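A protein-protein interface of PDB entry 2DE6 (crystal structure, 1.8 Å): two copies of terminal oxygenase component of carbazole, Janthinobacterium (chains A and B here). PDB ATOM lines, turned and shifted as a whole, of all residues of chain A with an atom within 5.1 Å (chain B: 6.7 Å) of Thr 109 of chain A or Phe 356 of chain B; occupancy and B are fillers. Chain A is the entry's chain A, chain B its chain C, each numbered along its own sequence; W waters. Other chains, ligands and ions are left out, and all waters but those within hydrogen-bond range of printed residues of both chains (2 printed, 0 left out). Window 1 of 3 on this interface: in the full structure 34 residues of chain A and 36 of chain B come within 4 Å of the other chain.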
ATOM      1  N   HIS A  71     -21.009 -22.349   9.436  1.00  0.00           N
ATOM      2  CA  HIS A  71     -21.230 -21.781  10.754  1.00  0.00           C
ATOM      3  C   HIS A  71     -22.555 -22.130  11.435  1.00  0.00           C
ATOM      4  O   HIS A  71     -22.587 -22.989  12.317  1.00  0.00           O
ATOM      5  CB  HIS A  71     -21.070 -20.263  10.666  1.00  0.00           C
ATOM      6  CG  HIS A  71     -21.054 -19.579  11.997  1.00  0.00           C
ATOM      7  ND1 HIS A  71     -21.556 -18.310  12.181  1.00  0.00           N
ATOM      8  CD2 HIS A  71     -20.584 -19.980  13.203  1.00  0.00           C
ATOM      9  CE1 HIS A  71     -21.396 -17.957  13.446  1.00  0.00           C
ATOM     10  NE2 HIS A  71     -20.808 -18.951  14.087  1.00  0.00           N
ATOM     11  N   HIS A  93     -22.493 -13.788   9.443  1.00  0.00           N
ATOM     12  CA  HIS A  93     -21.287 -13.367  10.157  1.00  0.00           C
ATOM     13  C   HIS A  93     -20.097 -13.211   9.219  1.00  0.00           C
ATOM     14  O   HIS A  93     -18.940 -13.244   9.642  1.00  0.00           O
ATOM     15  CB  HIS A  93     -20.942 -14.344  11.288  1.00  0.00           C
ATOM     16  CG  HIS A  93     -22.118 -14.735  12.127  1.00  0.00           C
ATOM     17  ND1 HIS A  93     -22.972 -15.758  11.775  1.00  0.00           N
ATOM     18  CD2 HIS A  93     -22.588 -14.237  13.297  1.00  0.00           C
ATOM     19  CE1 HIS A  93     -23.915 -15.876  12.693  1.00  0.00           C
ATOM     20  NE2 HIS A  93     -23.705 -14.965  13.627  1.00  0.00           N
ATOM     21  N   ALA A  94     -20.399 -13.062   7.935  1.00  0.00           N
ATOM     22  CA  ALA A  94     -19.389 -12.831   6.908  1.00  0.00           C
ATOM     23  C   ALA A  94     -18.301 -13.876   6.671  1.00  0.00           C
ATOM     24  O   ALA A  94     -17.198 -13.529   6.249  1.00  0.00           O
ATOM     25  CB  ALA A  94     -18.739 -11.466   7.142  1.00  0.00           C
ATOM     26  N   TRP A  95     -18.586 -15.146   6.942  1.00  0.00           N
ATOM     27  CA  TRP A  95     -17.600 -16.183   6.648  1.00  0.00           C
ATOM     28  C   TRP A  95     -17.513 -16.143   5.122  1.00  0.00           C
ATOM     29  O   TRP A  95     -18.535 -16.150   4.437  1.00  0.00           O
ATOM     30  CB  TRP A  95     -18.095 -17.548   7.135  1.00  0.00           C
ATOM     31  CG  TRP A  95     -17.923 -17.753   8.610  1.00  0.00           C
ATOM     32  CD1 TRP A  95     -18.018 -16.805   9.590  1.00  0.00           C
ATOM     33  CD2 TRP A  95     -17.671 -18.995   9.280  1.00  0.00           C
ATOM     34  NE1 TRP A  95     -17.844 -17.378  10.826  1.00  0.00           N
ATOM     35  CE2 TRP A  95     -17.630 -18.722  10.665  1.00  0.00           C
ATOM     36  CE3 TRP A  95     -17.478 -20.312   8.842  1.00  0.00           C
ATOM     37  CZ2 TRP A  95     -17.402 -19.722  11.621  1.00  0.00           C
ATOM     38  CZ3 TRP A  95     -17.249 -21.307   9.792  1.00  0.00           C
ATOM     39  CH2 TRP A  95     -17.215 -21.004  11.165  1.00  0.00           C
ATOM     40  N   ILE A 107     -12.943 -14.095   7.164  1.00  0.00           N
ATOM     41  CA  ILE A 107     -14.126 -13.929   8.005  1.00  0.00           C
ATOM     42  C   ILE A 107     -14.116 -12.449   8.363  1.00  0.00           C
ATOM     43  O   ILE A 107     -13.345 -12.014   9.218  1.00  0.00           O
ATOM     44  CB  ILE A 107     -14.073 -14.761   9.297  1.00  0.00           C
ATOM     45  CG1 ILE A 107     -14.061 -16.256   8.962  1.00  0.00           C
ATOM     46  CG2 ILE A 107     -15.299 -14.439  10.157  1.00  0.00           C
ATOM     47  CD1 ILE A 107     -13.972 -17.166  10.189  1.00  0.00           C
ATOM     48  N   LEU A 108     -14.961 -11.672   7.693  1.00  0.00           N
ATOM     49  CA  LEU A 108     -14.987 -10.233   7.926  1.00  0.00           C
ATOM     50  C   LEU A 108     -15.232  -9.805   9.366  1.00  0.00           C
ATOM     51  O   LEU A 108     -14.694  -8.789   9.804  1.00  0.00           O
ATOM     52  CB  LEU A 108     -16.015  -9.561   7.007  1.00  0.00           C
ATOM     53  CG  LEU A 108     -15.581  -9.323   5.556  1.00  0.00           C
ATOM     54  CD1 LEU A 108     -15.247 -10.629   4.868  1.00  0.00           C
ATOM     55  CD2 LEU A 108     -16.696  -8.598   4.823  1.00  0.00           C
ATOM     56  N   THR A 109     -16.030 -10.574  10.103  1.00  0.00           N
ATOM     57  CA  THR A 109     -16.336 -10.232  11.491  1.00  0.00           C
ATOM     58  C   THR A 109     -15.230 -10.570  12.498  1.00  0.00           C
ATOM     59  O   THR A 109     -15.327 -10.218  13.672  1.00  0.00           O
ATOM     60  CB  THR A 109     -17.629 -10.911  11.942  1.00  0.00           C
ATOM     61  OG1 THR A 109     -17.519 -12.326  11.736  1.00  0.00           O
ATOM     62  CG2 THR A 109     -18.815 -10.356  11.151  1.00  0.00           C
ATOM     63  N   ASN A 110     -14.191 -11.264  12.044  1.00  0.00           N
ATOM     64  CA  ASN A 110     -13.064 -11.617  12.911  1.00  0.00           C
ATOM     65  C   ASN A 110     -11.908 -12.111  12.051  1.00  0.00           C
ATOM     66  O   ASN A 110     -11.713 -13.316  11.878  1.00  0.00           O
ATOM     67  CB  ASN A 110     -13.455 -12.706  13.920  1.00  0.00           C
ATOM     68  CG  ASN A 110     -12.327 -13.036  14.888  1.00  0.00           C
ATOM     69  OD1 ASN A 110     -12.424 -13.972  15.688  1.00  0.00           O
ATOM     70  ND2 ASN A 110     -11.248 -12.262  14.822  1.00  0.00           N
ATOM     71  N   PRO A 111     -11.121 -11.177  11.499  1.00  0.00           N
ATOM     72  CA  PRO A 111      -9.980 -11.522  10.647  1.00  0.00           C
ATOM     73  C   PRO A 111      -8.870 -12.303  11.354  1.00  0.00           C
ATOM     74  O   PRO A 111      -7.930 -12.769  10.714  1.00  0.00           O
ATOM     75  CB  PRO A 111      -9.513 -10.161  10.135  1.00  0.00           C
ATOM     76  CG  PRO A 111      -9.841  -9.244  11.280  1.00  0.00           C
ATOM     77  CD  PRO A 111     -11.226  -9.717  11.678  1.00  0.00           C
ATOM     78  N   SER A 113      -9.626 -14.965  13.323  1.00  0.00           N
ATOM     79  CA  SER A 113     -10.168 -16.274  13.671  1.00  0.00           C
ATOM     80  C   SER A 113      -9.267 -17.431  13.250  1.00  0.00           C
ATOM     81  O   SER A 113      -8.719 -17.442  12.145  1.00  0.00           O
ATOM     82  CB  SER A 113     -11.546 -16.470  13.040  1.00  0.00           C
ATOM     83  OG  SER A 113     -12.037 -17.760  13.354  1.00  0.00           O
ATOM     84  N   GLN A 115     -10.266 -20.259  12.578  1.00  0.00           N
ATOM     85  CA  GLN A 115     -11.006 -21.096  11.632  1.00  0.00           C
ATOM     86  C   GLN A 115     -10.617 -20.791  10.186  1.00  0.00           C
ATOM     87  O   GLN A 115     -10.795 -21.620   9.293  1.00  0.00           O
ATOM     88  CB  GLN A 115     -12.516 -20.892  11.811  1.00  0.00           C
ATOM     89  CG  GLN A 115     -13.069 -21.473  13.107  1.00  0.00           C
ATOM     90  CD  GLN A 115     -13.110 -22.996  13.093  1.00  0.00           C
ATOM     91  OE1 GLN A 115     -12.196 -23.650  12.592  1.00  0.00           O
ATOM     92  NE2 GLN A 115     -14.173 -23.565  13.659  1.00  0.00           N
ATOM     93  N   ASP B 180     -25.630 -12.852  19.996  1.00  0.00           N
ATOM     94  CA  ASP B 180     -24.514 -13.155  19.097  1.00  0.00           C
ATOM     95  C   ASP B 180     -23.674 -11.896  18.835  1.00  0.00           C
ATOM     96  O   ASP B 180     -24.105 -11.005  18.109  1.00  0.00           O
ATOM     97  CB  ASP B 180     -25.110 -13.677  17.786  1.00  0.00           C
ATOM     98  CG  ASP B 180     -24.081 -14.268  16.859  1.00  0.00           C
ATOM     99  OD1 ASP B 180     -22.935 -13.771  16.824  1.00  0.00           O
ATOM    100  OD2 ASP B 180     -24.443 -15.230  16.148  1.00  0.00           O
ATOM    101  N   SER B 182     -21.010 -11.256  16.913  1.00  0.00           N
ATOM    102  CA  SER B 182     -20.700 -11.021  15.509  1.00  0.00           C
ATOM    103  C   SER B 182     -21.869 -10.828  14.547  1.00  0.00           C
ATOM    104  O   SER B 182     -21.652 -10.417  13.410  1.00  0.00           O
ATOM    105  CB  SER B 182     -19.799 -12.145  14.987  1.00  0.00           C
ATOM    106  OG  SER B 182     -18.559 -12.167  15.677  1.00  0.00           O
ATOM    107  N   HIS B 183     -23.100 -11.100  14.974  1.00  0.00           N
ATOM    108  CA  HIS B 183     -24.220 -10.937  14.048  1.00  0.00           C
ATOM    109  C   HIS B 183     -24.464  -9.467  13.727  1.00  0.00           C
ATOM    110  O   HIS B 183     -25.262  -9.138  12.856  1.00  0.00           O
ATOM    111  CB  HIS B 183     -25.505 -11.581  14.602  1.00  0.00           C
ATOM    112  CG  HIS B 183     -26.359 -10.654  15.408  1.00  0.00           C
ATOM    113  ND1 HIS B 183     -26.022 -10.243  16.678  1.00  0.00           N
ATOM    114  CD2 HIS B 183     -27.539 -10.053  15.119  1.00  0.00           C
ATOM    115  CE1 HIS B 183     -26.955  -9.430  17.139  1.00  0.00           C
ATOM    116  NE2 HIS B 183     -27.886  -9.298  16.212  1.00  0.00           N
ATOM    117  N   ILE B 184     -23.763  -8.588  14.432  1.00  0.00           N
ATOM    118  CA  ILE B 184     -23.904  -7.154  14.217  1.00  0.00           C
ATOM    119  C   ILE B 184     -23.701  -6.840  12.730  1.00  0.00           C
ATOM    120  O   ILE B 184     -24.174  -5.818  12.219  1.00  0.00           O
ATOM    121  CB  ILE B 184     -22.881  -6.391  15.085  1.00  0.00           C
ATOM    122  CG1 ILE B 184     -23.168  -4.894  15.050  1.00  0.00           C
ATOM    123  CG2 ILE B 184     -21.472  -6.704  14.613  1.00  0.00           C
ATOM    124  CD1 ILE B 184     -22.281  -4.098  15.987  1.00  0.00           C
ATOM    125  N   TYR B 185     -23.002  -7.737  12.042  1.00  0.00           N
ATOM    126  CA  TYR B 185     -22.735  -7.601  10.613  1.00  0.00           C
ATOM    127  C   TYR B 185     -24.019  -7.453   9.782  1.00  0.00           C
ATOM    128  O   TYR B 185     -24.031  -6.751   8.770  1.00  0.00           O
ATOM    129  CB  TYR B 185     -21.960  -8.827  10.117  1.00  0.00           C
ATOM    130  CG  TYR B 185     -21.567  -8.765   8.658  1.00  0.00           C
ATOM    131  CD1 TYR B 185     -20.533  -7.929   8.229  1.00  0.00           C
ATOM    132  CD2 TYR B 185     -22.238  -9.526   7.702  1.00  0.00           C
ATOM    133  CE1 TYR B 185     -20.180  -7.851   6.886  1.00  0.00           C
ATOM    134  CE2 TYR B 185     -21.894  -9.455   6.352  1.00  0.00           C
ATOM    135  CZ  TYR B 185     -20.865  -8.615   5.951  1.00  0.00           C
ATOM    136  OH  TYR B 185     -20.530  -8.524   4.620  1.00  0.00           O
ATOM    137  N   LEU B 202     -18.243  -3.808  12.274  1.00  0.00           N
ATOM    138  CA  LEU B 202     -18.721  -4.931  11.473  1.00  0.00           C
ATOM    139  C   LEU B 202     -18.582  -6.206  12.288  1.00  0.00           C
ATOM    140  O   LEU B 202     -19.231  -7.212  12.008  1.00  0.00           O
ATOM    141  CB  LEU B 202     -17.885  -5.074  10.202  1.00  0.00           C
ATOM    142  CG  LEU B 202     -17.957  -3.940   9.180  1.00  0.00           C
ATOM    143  CD1 LEU B 202     -16.941  -4.202   8.074  1.00  0.00           C
ATOM    144  CD2 LEU B 202     -19.366  -3.843   8.612  1.00  0.00           C
ATOM    145  N   GLY B 203     -17.713  -6.159  13.290  1.00  0.00           N
ATOM    146  CA  GLY B 203     -17.482  -7.324  14.122  1.00  0.00           C
ATOM    147  C   GLY B 203     -16.396  -7.054  15.137  1.00  0.00           C
ATOM    148  O   GLY B 203     -16.076  -5.895  15.410  1.00  0.00           O
ATOM    149  N   PHE B 204     -15.806  -8.117  15.676  1.00  0.00           N
ATOM    150  CA  PHE B 204     -14.773  -7.964  16.691  1.00  0.00           C
ATOM    151  C   PHE B 204     -13.653  -8.988  16.605  1.00  0.00           C
ATOM    152  O   PHE B 204     -13.882 -10.161  16.302  1.00  0.00           O
ATOM    153  CB  PHE B 204     -15.397  -8.087  18.083  1.00  0.00           C
ATOM    154  CG  PHE B 204     -16.594  -7.213  18.296  1.00  0.00           C
ATOM    155  CD1 PHE B 204     -16.448  -5.917  18.777  1.00  0.00           C
ATOM    156  CD2 PHE B 204     -17.873  -7.682  18.005  1.00  0.00           C
ATOM    157  CE1 PHE B 204     -17.557  -5.098  18.968  1.00  0.00           C
ATOM    158  CE2 PHE B 204     -18.987  -6.874  18.191  1.00  0.00           C
ATOM    159  CZ  PHE B 204     -18.831  -5.577  18.674  1.00  0.00           C
ATOM    160  N   ALA B 205     -12.437  -8.533  16.885  1.00  0.00           N
ATOM    161  CA  ALA B 205     -11.276  -9.414  16.924  1.00  0.00           C
ATOM    162  C   ALA B 205     -11.068  -9.576  18.430  1.00  0.00           C
ATOM    163  O   ALA B 205     -10.599  -8.654  19.097  1.00  0.00           O
ATOM    164  CB  ALA B 205     -10.064  -8.739  16.279  1.00  0.00           C
ATOM    165  N   PRO B 206     -11.447 -10.740  18.990  1.00  0.00           N
ATOM    166  CA  PRO B 206     -11.318 -11.036  20.422  1.00  0.00           C
ATOM    167  C   PRO B 206      -9.913 -10.892  20.992  1.00  0.00           C
ATOM    168  O   PRO B 206      -8.921 -11.052  20.283  1.00  0.00           O
ATOM    169  CB  PRO B 206     -11.821 -12.476  20.530  1.00  0.00           C
ATOM    170  CG  PRO B 206     -12.786 -12.584  19.399  1.00  0.00           C
ATOM    171  CD  PRO B 206     -12.048 -11.885  18.284  1.00  0.00           C
ATOM    172  N   VAL B 236     -10.481  -5.915  19.533  1.00  0.00           N
ATOM    173  CA  VAL B 236     -10.343  -4.771  18.648  1.00  0.00           C
ATOM    174  C   VAL B 236     -11.535  -4.794  17.698  1.00  0.00           C
ATOM    175  O   VAL B 236     -11.714  -5.748  16.943  1.00  0.00           O
ATOM    176  CB  VAL B 236      -9.043  -4.864  17.819  1.00  0.00           C
ATOM    177  CG1 VAL B 236      -8.993  -3.745  16.795  1.00  0.00           C
ATOM    178  CG2 VAL B 236      -7.835  -4.797  18.746  1.00  0.00           C
ATOM    179  N   VAL B 238     -13.880  -4.322  14.513  1.00  0.00           N
ATOM    180  CA  VAL B 238     -13.585  -4.358  13.087  1.00  0.00           C
ATOM    181  C   VAL B 238     -14.373  -3.292  12.341  1.00  0.00           C
ATOM    182  O   VAL B 238     -15.603  -3.315  12.333  1.00  0.00           O
ATOM    183  CB  VAL B 238     -13.943  -5.732  12.469  1.00  0.00           C
ATOM    184  CG1 VAL B 238     -13.624  -5.733  10.974  1.00  0.00           C
ATOM    185  CG2 VAL B 238     -13.186  -6.838  13.182  1.00  0.00           C
ATOM    186  N   GLY B 241     -13.588  -4.289   6.763  1.00  0.00           N
ATOM    187  CA  GLY B 241     -13.705  -5.698   6.425  1.00  0.00           C
ATOM    188  C   GLY B 241     -12.898  -6.006   5.180  1.00  0.00           C
ATOM    189  O   GLY B 241     -13.066  -5.351   4.149  1.00  0.00           O
ATOM    190  N   ILE B 354     -20.514 -25.344  13.139  1.00  0.00           N
ATOM    191  CA  ILE B 354     -19.070 -25.125  13.271  1.00  0.00           C
ATOM    192  C   ILE B 354     -18.930 -23.709  13.831  1.00  0.00           C
ATOM    193  O   ILE B 354     -19.130 -22.719  13.131  1.00  0.00           O
ATOM    194  CB  ILE B 354     -18.340 -25.257  11.918  1.00  0.00           C
ATOM    195  CG1 ILE B 354     -18.461 -26.704  11.417  1.00  0.00           C
ATOM    196  CG2 ILE B 354     -16.860 -24.891  12.079  1.00  0.00           C
ATOM    197  CD1 ILE B 354     -17.785 -26.968  10.086  1.00  0.00           C
ATOM    198  N   LEU B 355     -18.597 -23.623  15.111  1.00  0.00           N
ATOM    199  CA  LEU B 355     -18.496 -22.332  15.780  1.00  0.00           C
ATOM    200  C   LEU B 355     -17.145 -21.644  15.650  1.00  0.00           C
ATOM    201  O   LEU B 355     -16.145 -22.273  15.305  1.00  0.00           O
ATOM    202  CB  LEU B 355     -18.807 -22.510  17.274  1.00  0.00           C
ATOM    203  CG  LEU B 355     -20.087 -23.276  17.633  1.00  0.00           C
ATOM    204  CD1 LEU B 355     -20.240 -23.357  19.138  1.00  0.00           C
ATOM    205  CD2 LEU B 355     -21.287 -22.580  17.010  1.00  0.00           C
ATOM    206  N   PHE B 356     -17.126 -20.339  15.900  1.00  0.00           N
ATOM    207  CA  PHE B 356     -15.860 -19.624  15.906  1.00  0.00           C
ATOM    208  C   PHE B 356     -15.766 -18.807  17.190  1.00  0.00           C
ATOM    209  O   PHE B 356     -16.677 -18.849  18.015  1.00  0.00           O
ATOM    210  CB  PHE B 356     -15.609 -18.824  14.602  1.00  0.00           C
ATOM    211  CG  PHE B 356     -16.379 -17.541  14.453  1.00  0.00           C
ATOM    212  CD1 PHE B 356     -17.715 -17.436  14.819  1.00  0.00           C
ATOM    213  CD2 PHE B 356     -15.775 -16.458  13.809  1.00  0.00           C
ATOM    214  CE1 PHE B 356     -18.439 -16.270  14.537  1.00  0.00           C
ATOM    215  CE2 PHE B 356     -16.486 -15.296  13.522  1.00  0.00           C
ATOM    216  CZ  PHE B 356     -17.823 -15.201  13.886  1.00  0.00           C
ATOM    217  N   GLU B 357     -14.661 -18.097  17.380  1.00  0.00           N
ATOM    218  CA  GLU B 357     -14.411 -17.365  18.619  1.00  0.00           C
ATOM    219  C   GLU B 357     -15.520 -16.597  19.338  1.00  0.00           C
ATOM    220  O   GLU B 357     -15.748 -16.817  20.533  1.00  0.00           O
ATOM    221  CB  GLU B 357     -13.196 -16.454  18.431  1.00  0.00           C
ATOM    222  CG  GLU B 357     -11.879 -17.214  18.282  1.00  0.00           C
ATOM    223  CD  GLU B 357     -11.647 -17.742  16.877  1.00  0.00           C
ATOM    224  OE1 GLU B 357     -12.493 -17.488  15.996  1.00  0.00           O
ATOM    225  OE2 GLU B 357     -10.609 -18.404  16.650  1.00  0.00           O
ATOM    226  N   SER B 358     -16.213 -15.704  18.641  1.00  0.00           N
ATOM    227  CA  SER B 358     -17.256 -14.919  19.290  1.00  0.00           C
ATOM    228  C   SER B 358     -18.415 -15.743  19.836  1.00  0.00           C
ATOM    229  O   SER B 358     -19.182 -15.263  20.672  1.00  0.00           O
ATOM    230  CB  SER B 358     -17.784 -13.834  18.341  1.00  0.00           C
ATOM    231  OG  SER B 358     -18.295 -14.385  17.141  1.00  0.00           O
ATOM    232  N   ASP B 359     -18.543 -16.986  19.381  1.00  0.00           N
ATOM    233  CA  ASP B 359     -19.623 -17.835  19.865  1.00  0.00           C
ATOM    234  C   ASP B 359     -19.397 -18.235  21.315  1.00  0.00           C
ATOM    235  O   ASP B 359     -20.221 -18.921  21.917  1.00  0.00           O
ATOM    236  CB  ASP B 359     -19.769 -19.075  18.977  1.00  0.00           C
ATOM    237  CG  ASP B 359     -20.218 -18.725  17.572  1.00  0.00           C
ATOM    238  OD1 ASP B 359     -21.087 -17.832  17.435  1.00  0.00           O
ATOM    239  OD2 ASP B 359     -19.717 -19.342  16.607  1.00  0.00           O
ATOM    240  N   GLU B 360     -18.277 -17.796  21.880  1.00  0.00           N
ATOM    241  CA  GLU B 360     -17.971 -18.099  23.268  1.00  0.00           C
ATOM    242  C   GLU B 360     -19.116 -17.559  24.131  1.00  0.00           C
ATOM    243  O   GLU B 360     -19.471 -18.141  25.160  1.00  0.00           O
ATOM    244  CB  GLU B 360     -16.649 -17.438  23.667  1.00  0.00           C
ATOM    245  CG  GLU B 360     -15.968 -18.096  24.848  1.00  0.00           C
ATOM    246  CD  GLU B 360     -15.600 -19.548  24.573  1.00  0.00           C
ATOM    247  OE1 GLU B 360     -14.656 -19.804  23.785  1.00  0.00           O
ATOM    248  OE2 GLU B 360     -16.266 -20.433  25.141  1.00  0.00           O
HETATM  249  O   HOH W   1     -15.841 -11.952  16.380  1.00  0.00           O
HETATM  250  O   HOH W   2     -15.076 -14.577  16.281  1.00  0.00           O
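Of the 20 printed residues of chain B, 15 touch a printed residue of chain A.
Hydrophobic or aromatic side chains of chain B that line the printed part of chain A: His 183, Tyr 185, Ala 205, Pro 206, Val 238, Ile 354 and Phe 356.
Of the 11 printed residues of chain A, 11 touch a printed residue of chain B.
Hydrophobic or aromatic side chains of chain A within 4 Å of the printed part of chain B: His 71, His 93, Ala 94, Trp 95, Ile 107, Leu 108 and Pro 111.
Along chain A the printed residues that touch a printed residue of chain B span positions 71 to 115.
Among the printed residues, 28 pairs touch across the chains.
Of chain B, only Ser 182 (3.6 Å), Tyr 185 (3.6 Å), Leu 202 (3.3 Å), Gly 203 (3.6 Å), Phe 204 (2.9 Å) and Phe 356 (3.6 Å) come within 4 Å of Thr 109 of chain A.
Of the printed residues of chain B, Ile 107 of chain A touches Phe 356.
Of the printed residues of chain A, Ile 354 of chain B touches His 71 (3.1 Å), Trp 95 (3.2 Å) and Gln 115 (3.4 Å).
Val 236 of chain B touches none of the printed residues of chain A.
The nearest residue of chain B that does not touch Thr 109 of chain A is Val 238 of chain B (4.03 Å).
The nearest printed residue of chain A that does not touch Phe 356 of chain B is Asn 110 of chain A (4.01 Å).
The backbone carbonyl oxygen (O) of His 93 of chain A lies within hydrogen-bond range of the side-chain hydroxyl (OG1) of Thr 109 of chain A.
OG of Ser 113 of chain A sits close to N of Gln 115 of chain A, at 3.2 Å.
The backbone carbonyl oxygen (O) of Asp 180 of chain B lies within hydrogen-bond range of a ring nitrogen (ND1) of His 183 of chain B (2.5 Å).
The side-chain hydroxyl (OG) of Ser 182 of chain B is in hydrogen-bond range of the side-chain hydroxyl (OG) of Ser 358 of chain B (2.7 Å).
The backbone carbonyl oxygen (O) of Ala 205 of chain B lies within hydrogen-bond range of the backbone NH (N) of Val 236 of chain B (2.8 Å).
OD2 of Asp 359 of chain B sits at hydrogen-bond distance from N of Phe 356 of chain B (2.9 Å).
The backbone carbonyl oxygen of His 71 of chain A sits at hydrogen-bond distance from the backbone NH of Ile 354 of chain B (3.2 Å).
NE2 of His 71 of chain A sits at hydrogen-bond distance from OD2 of Asp 359 of chain B (2.8 Å).
OD2 of Asp 180 of chain B is in hydrogen-bond range of NE2 of His 93 of chain A (2.6 Å).
The backbone carbonyl oxygen (O) of Thr 109 of chain A sits at hydrogen-bond distance from the backbone NH (N) of Phe 204 of chain B, 2.9 Å away.
OE1 of Glu 357 of chain B lies within hydrogen-bond range of OG of Ser 113 of chain A, 2.7 Å away.
The side-chain amide nitrogen (NE2) of Gln 115 of chain A sits at hydrogen-bond distance from the backbone carbonyl oxygen (O) of Leu 355 of chain B.
Water W1 lies within hydrogen-bond range of O of Phe 204 of chain B (2.7 Å), OG of Ser 182 of chain B (2.8 Å) and O of Thr 109 of chain A (3.3 Å).
Water W2 bridges the side-chain amide oxygen (OD1) of Asn 110 of chain A (2.8 Å) and the backbone NH (N) of Ser 358 of chain B (2.9 Å).
Among the printed residues, merely in contact across the chains: Trp 95 of chain A with Ile 354 of chain B (3.2 Å), Thr 109 of chain A with Leu 202 of chain B (3.3 Å), Asn 110 of chain A with Pro 206 of chain B (3.4 Å), Gln 115 of chain A with Ile 354 of chain B (3.4 Å), Leu 108 of chain A with Val 238 of chain B (3.4 Å), Asn 110 of chain A with Phe 204 of chain B (3.5 Å), His 71 of chain A with Phe 356 of chain B (3.5 Å), Asn 110 of chain A with Glu 357 of chain B (3.5 Å), Asn 110 of chain A with Ala 205 of chain B (3.5 Å), Trp 95 of chain A with Phe 356 of chain B (3.6 Å), His 93 of chain A with His 183 of chain B (3.6 Å), Thr 109 of chain A with Phe 356 of chain B (3.6 Å), Thr 109 of chain A with Ser 182 of chain B (3.6 Å), Thr 109 of chain A with Gly 203 of chain B (3.6 Å), Thr 109 of chain A with Tyr 185 of chain B (3.6 Å), Ile 107 of chain A with Phe 356 of chain B (3.7 Å), His 93 of chain A with Ser 182 of chain B (3.7 Å), Ala 94 of chain A with Tyr 185 of chain B (3.8 Å), Pro 111 of chain A with Val 238 of chain B (3.8 Å), Leu 108 of chain A with Tyr 185 of chain B (3.8 Å), Ser 113 of chain A with Phe 356 of chain B (3.9 Å) and Gln 115 of chain A with Phe 356 of chain B (3.96 Å).
No position is printed for both chains.
Of the 28 pairs that touch across the chains among the printed residues, none has its exchanged pair printed and touching as well.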
